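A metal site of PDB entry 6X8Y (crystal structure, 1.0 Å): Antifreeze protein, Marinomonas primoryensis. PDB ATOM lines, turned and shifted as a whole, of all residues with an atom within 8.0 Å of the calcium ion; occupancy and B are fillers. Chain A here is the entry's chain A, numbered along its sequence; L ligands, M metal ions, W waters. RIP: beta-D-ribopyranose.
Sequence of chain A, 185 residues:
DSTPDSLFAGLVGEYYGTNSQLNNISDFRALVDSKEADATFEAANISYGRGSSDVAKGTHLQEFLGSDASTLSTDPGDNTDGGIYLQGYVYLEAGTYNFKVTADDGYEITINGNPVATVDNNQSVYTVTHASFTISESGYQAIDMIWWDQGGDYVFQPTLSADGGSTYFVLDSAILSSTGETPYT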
ATOM      1  N   THR A  18     -25.451   5.433 -16.175  1.00  0.00           N
ATOM      2  CA  THR A  18     -26.907   5.307 -16.167  1.00  0.00           C
ATOM      3  C   THR A  18     -27.500   6.254 -17.177  1.00  0.00           C
ATOM      4  O   THR A  18     -26.888   7.271 -17.539  1.00  0.00           O
ATOM      5  CB  THR A  18     -27.469   5.590 -14.742  1.00  0.00           C
ATOM      6  OG1 THR A  18     -28.876   5.390 -14.710  1.00  0.00           O
ATOM      7  CG2 THR A  18     -27.230   7.016 -14.290  1.00  0.00           C
ATOM      8  N   ASN A  19     -28.718   5.936 -17.624  1.00  0.00           N
ATOM      9  CA  ASN A  19     -29.493   6.862 -18.446  1.00  0.00           C
ATOM     10  C   ASN A  19     -30.595   7.582 -17.695  1.00  0.00           C
ATOM     11  O   ASN A  19     -31.455   8.247 -18.295  1.00  0.00           O
ATOM     12  CB  ASN A  19     -30.040   6.160 -19.685  1.00  0.00           C
ATOM     13  CG  ASN A  19     -28.897   5.576 -20.489  1.00  0.00           C
ATOM     14  OD1 ASN A  19     -27.841   6.226 -20.683  1.00  0.00           O
ATOM     15  ND2 ASN A  19     -29.043   4.353 -20.963  1.00  0.00           N
ATOM     16  N   SER A  20     -30.582   7.438 -16.360  1.00  0.00           N
ATOM     17  CA  SER A  20     -31.382   8.238 -15.458  1.00  0.00           C
ATOM     18  C   SER A  20     -30.586   9.444 -14.976  1.00  0.00           C
ATOM     19  O   SER A  20     -29.355   9.486 -15.110  1.00  0.00           O
ATOM     20  CB  SER A  20     -31.823   7.369 -14.279  1.00  0.00           C
ATOM     21  OG  SER A  20     -30.736   7.066 -13.408  1.00  0.00           O
ATOM     22  N   GLN A  21     -31.296  10.436 -14.425  1.00  0.00           N
ATOM     23  CA  GLN A  21     -30.652  11.656 -13.945  1.00  0.00           C
ATOM     24  C   GLN A  21     -30.052  11.457 -12.555  1.00  0.00           C
ATOM     25  O   GLN A  21     -30.705  10.975 -11.626  1.00  0.00           O
ATOM     26  CB  GLN A  21     -31.682  12.785 -13.903  1.00  0.00           C
ATOM     27  CG  GLN A  21     -31.251  14.012 -13.141  1.00  0.00           C
ATOM     28  CD  GLN A  21     -30.111  14.808 -13.788  1.00  0.00           C
ATOM     29  OE1 GLN A  21     -29.499  14.386 -14.771  1.00  0.00           O
ATOM     30  NE2 GLN A  21     -29.846  16.004 -13.247  1.00  0.00           N
ATOM     31  N   LEU A  22     -28.823  11.901 -12.410  1.00  0.00           N
ATOM     32  CA  LEU A  22     -28.154  11.984 -11.106  1.00  0.00           C
ATOM     33  C   LEU A  22     -28.245  13.427 -10.606  1.00  0.00           C
ATOM     34  O   LEU A  22     -27.610  14.321 -11.180  1.00  0.00           O
ATOM     35  CB  LEU A  22     -26.698  11.537 -11.240  1.00  0.00           C
ATOM     36  CG  LEU A  22     -26.496  10.072 -11.662  1.00  0.00           C
ATOM     37  CD1 LEU A  22     -25.017   9.802 -11.891  1.00  0.00           C
ATOM     38  CD2 LEU A  22     -27.104   9.089 -10.666  1.00  0.00           C
ATOM     39  N   ASN A  23     -29.019  13.660  -9.536  1.00  0.00           N
ATOM     40  CA  ASN A  23     -29.197  14.991  -8.968  1.00  0.00           C
ATOM     41  C   ASN A  23     -28.408  15.215  -7.694  1.00  0.00           C
ATOM     42  O   ASN A  23     -28.225  16.373  -7.293  1.00  0.00           O
ATOM     43  CB  ASN A  23     -30.682  15.255  -8.639  1.00  0.00           C
ATOM     44  CG  ASN A  23     -31.486  15.588  -9.865  1.00  0.00           C
ATOM     45  OD1 ASN A  23     -31.083  16.439 -10.663  1.00  0.00           O
ATOM     46  ND2 ASN A  23     -32.641  14.960 -10.010  1.00  0.00           N
ATOM     47  N   ASP A  54     -20.041  15.107 -21.557  1.00  0.00           N
ATOM     48  CA  ASP A  54     -20.569  13.989 -20.720  1.00  0.00           C
ATOM     49  C   ASP A  54     -19.491  12.953 -20.394  1.00  0.00           C
ATOM     50  O   ASP A  54     -18.942  12.287 -21.304  1.00  0.00           O
ATOM     51  CB  ASP A  54     -21.796  13.249 -21.297  1.00  0.00           C
ATOM     52  CG  ASP A  54     -22.897  14.123 -21.876  1.00  0.00           C
ATOM     53  OD1 ASP A  54     -23.175  15.203 -21.334  1.00  0.00           O
ATOM     54  OD2 ASP A  54     -23.570  13.629 -22.832  1.00  0.00           O
ATOM     55  N   THR A  80     -25.864   8.523 -20.341  1.00  0.00           N
ATOM     56  CA  THR A  80     -25.971   9.980 -20.229  1.00  0.00           C
ATOM     57  C   THR A  80     -25.271  10.524 -18.973  1.00  0.00           C
ATOM     58  O   THR A  80     -24.721  11.643 -19.020  1.00  0.00           O
ATOM     59  CB  THR A  80     -27.447  10.434 -20.232  1.00  0.00           C
ATOM     60  OG1 THR A  80     -28.133   9.958 -19.060  1.00  0.00           O
ATOM     61  CG2 THR A  80     -28.189   9.910 -21.452  1.00  0.00           C
ATOM     62  N   ASP A  81     -25.290   9.756 -17.892  1.00  0.00           N
ATOM     63  CA  ASP A  81     -24.824  10.183 -16.588  1.00  0.00           C
ATOM     64  C   ASP A  81     -23.901   9.098 -16.049  1.00  0.00           C
ATOM     65  O   ASP A  81     -24.040   7.924 -16.412  1.00  0.00           O
ATOM     66  CB  ASP A  81     -26.025  10.334 -15.609  1.00  0.00           C
ATOM     67  CG  ASP A  81     -26.973  11.482 -15.925  1.00  0.00           C
ATOM     68  OD1 ASP A  81     -27.419  11.607 -17.090  1.00  0.00           O
ATOM     69  OD2 ASP A  81     -27.304  12.279 -14.999  1.00  0.00           O
ATOM     70  N   GLY A  82     -22.968   9.465 -15.177  1.00  0.00           N
ATOM     71  CA  GLY A  82     -22.125   8.414 -14.610  1.00  0.00           C
ATOM     72  C   GLY A  82     -21.261   8.955 -13.498  1.00  0.00           C
ATOM     73  O   GLY A  82     -21.190  10.162 -13.281  1.00  0.00           O
ATOM     74  N   ASP A 105     -19.689  17.116 -11.219  1.00  0.00           N
ATOM     75  CA  ASP A 105     -20.781  17.701 -10.417  1.00  0.00           C
ATOM     76  C   ASP A 105     -20.420  17.567  -8.928  1.00  0.00           C
ATOM     77  O   ASP A 105     -19.442  18.176  -8.499  1.00  0.00           O
ATOM     78  CB  ASP A 105     -22.121  17.090 -10.837  1.00  0.00           C
ATOM     79  CG  ASP A 105     -22.592  17.673 -12.145  1.00  0.00           C
ATOM     80  OD1 ASP A 105     -23.108  18.828 -12.099  1.00  0.00           O
ATOM     81  OD2 ASP A 105     -22.413  17.057 -13.234  1.00  0.00           O
ATOM     82  N   ASN A 122     -25.722  19.046  -8.086  1.00  0.00           N
ATOM     83  CA  ASN A 122     -25.029  19.315  -9.322  1.00  0.00           C
ATOM     84  C   ASN A 122     -24.449  20.721  -9.308  1.00  0.00           C
ATOM     85  O   ASN A 122     -24.919  21.604  -8.593  1.00  0.00           O
ATOM     86  CB  ASN A 122     -25.933  19.082 -10.524  1.00  0.00           C
ATOM     87  CG  ASN A 122     -26.223  17.625 -10.728  1.00  0.00           C
ATOM     88  OD1 ASN A 122     -25.336  16.801 -10.524  1.00  0.00           O
ATOM     89  ND2 ASN A 122     -27.439  17.294 -11.150  1.00  0.00           N
ATOM     90  N   TRP A 148     -19.883  12.253  -9.223  1.00  0.00           N
ATOM     91  CA  TRP A 148     -20.608  11.952 -10.444  1.00  0.00           C
ATOM     92  C   TRP A 148     -20.679  13.174 -11.351  1.00  0.00           C
ATOM     93  O   TRP A 148     -20.407  14.310 -10.942  1.00  0.00           O
ATOM     94  CB  TRP A 148     -22.057  11.444 -10.120  1.00  0.00           C
ATOM     95  CG  TRP A 148     -22.990  12.540  -9.681  1.00  0.00           C
ATOM     96  CD1 TRP A 148     -23.794  13.282 -10.490  1.00  0.00           C
ATOM     97  CD2 TRP A 148     -23.113  13.117  -8.377  1.00  0.00           C
ATOM     98  NE1 TRP A 148     -24.426  14.284  -9.788  1.00  0.00           N
ATOM     99  CE2 TRP A 148     -24.023  14.194  -8.485  1.00  0.00           C
ATOM    100  CE3 TRP A 148     -22.573  12.793  -7.126  1.00  0.00           C
ATOM    101  CZ2 TRP A 148     -24.370  14.989  -7.394  1.00  0.00           C
ATOM    102  CZ3 TRP A 148     -22.923  13.591  -6.056  1.00  0.00           C
ATOM    103  CH2 TRP A 148     -23.804  14.668  -6.182  1.00  0.00           C
ATOM    104  N   ASP A 149     -21.104  12.876 -12.577  1.00  0.00           N
ATOM    105  CA  ASP A 149     -21.420  13.840 -13.624  1.00  0.00           C
ATOM    106  C   ASP A 149     -22.861  13.589 -14.074  1.00  0.00           C
ATOM    107  O   ASP A 149     -23.205  12.484 -14.519  1.00  0.00           O
ATOM    108  CB  ASP A 149     -20.479  13.652 -14.822  1.00  0.00           C
ATOM    109  CG  ASP A 149     -20.824  14.562 -15.974  1.00  0.00           C
ATOM    110  OD1 ASP A 149     -21.246  15.704 -15.709  1.00  0.00           O
ATOM    111  OD2 ASP A 149     -20.743  14.123 -17.152  1.00  0.00           O
ATOM    112  N   GLN A 150     -23.696  14.629 -13.983  1.00  0.00           N
ATOM    113  CA  GLN A 150     -25.061  14.573 -14.545  1.00  0.00           C
ATOM    114  C   GLN A 150     -25.068  14.773 -16.050  1.00  0.00           C
ATOM    115  O   GLN A 150     -26.119  14.595 -16.688  1.00  0.00           O
ATOM    116  CB  GLN A 150     -25.979  15.620 -13.878  1.00  0.00           C
ATOM    117  CG  GLN A 150     -25.640  17.061 -14.261  1.00  0.00           C
ATOM    118  CD  GLN A 150     -26.813  18.016 -14.291  1.00  0.00           C
ATOM    119  OE1 GLN A 150     -27.948  17.654 -14.613  1.00  0.00           O
ATOM    120  NE2 GLN A 150     -26.524  19.288 -13.973  1.00  0.00           N
ATOM    121  N   GLY A 151     -23.938  15.188 -16.626  1.00  0.00           N
ATOM    122  CA  GLY A 151     -23.834  15.574 -18.012  1.00  0.00           C
ATOM    123  C   GLY A 151     -23.077  16.860 -18.160  1.00  0.00           C
ATOM    124  O   GLY A 151     -22.889  17.640 -17.197  1.00  0.00           O
ATOM    125  N   GLY A 152     -22.624  17.110 -19.378  1.00  0.00           N
ATOM    126  CA  GLY A 152     -21.886  18.338 -19.697  1.00  0.00           C
ATOM    127  C   GLY A 152     -20.427  18.232 -19.362  1.00  0.00           C
ATOM    128  O   GLY A 152     -19.751  17.279 -19.789  1.00  0.00           O
HETATM  129  C1  RIP L   1     -23.305  21.143 -17.096  1.00  0.00           C
HETATM  130  C2  RIP L   1     -22.249  21.211 -16.015  1.00  0.00           C
HETATM  131  C3  RIP L   1     -22.864  20.973 -14.657  1.00  0.00           C
HETATM  132  C4  RIP L   1     -24.047  21.884 -14.424  1.00  0.00           C
HETATM  133  C5  RIP L   1     -24.987  21.796 -15.600  1.00  0.00           C
HETATM  134  O1  RIP L   1     -22.750  21.496 -18.338  1.00  0.00           O
HETATM  135  O2  RIP L   1     -21.201  20.285 -16.289  1.00  0.00           O
HETATM  136  O3  RIP L   1     -23.250  19.589 -14.583  1.00  0.00           O
HETATM  137  O4  RIP L   1     -24.692  21.484 -13.232  1.00  0.00           O
HETATM  138  O5  RIP L   1     -24.304  22.126 -16.788  1.00  0.00           O
HETATM  139 CA    CA M   1     -28.330  13.817 -16.683  1.00  0.00          CA
HETATM  140  O   HOH W   1     -30.439  12.998 -17.161  1.00  0.00           O
HETATM  141  O   HOH W   2     -28.238  14.119 -19.082  1.00  0.00           O
HETATM  142  O   HOH W   3     -28.646  16.202 -16.953  1.00  0.00           O
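The side-chain amide nitrogen (NE2) of Gln 150 sits at hydrogen-bond distance from an oxygen (O4) of the ligand (3.0 Å).
The side-chain amide nitrogen (ND2) of Asn 122 sits close to the side-chain amide nitrogen (NE2) of Gln 21, at 3.4 Å.
The side-chain amide oxygen (OD1) of Asn 23 sits at hydrogen-bond distance from the side-chain amide nitrogen (NE2) of Gln 21 (2.9 Å).
N of Gln 150 lies close to OD2 of Asp 105 (2.8 Å).
OD1 of Asp 81 sits close to OG1 of Thr 80, at 2.7 Å.
N of Leu 22 sits close to OD2 of Asp 81 (3.0 Å).
O of Asp 81 lies within hydrogen-bond range of N of Thr 18 (2.9 Å).
Of the 17 residues printed, 3 come within 4 Å of the calcium ion.
The calcium ion is bound by OE1 of Gln 21 (2.3 Å), water W1 (2.3 Å), O of Gln 150 (2.3 Å), water W2 (2.4 Å), water W3 (2.4 Å), OD1 of Asp 81 (2.4 Å) and OD2 of Asp 81 (2.5 Å).
The calcium ion has seven donor atoms within binding distance.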
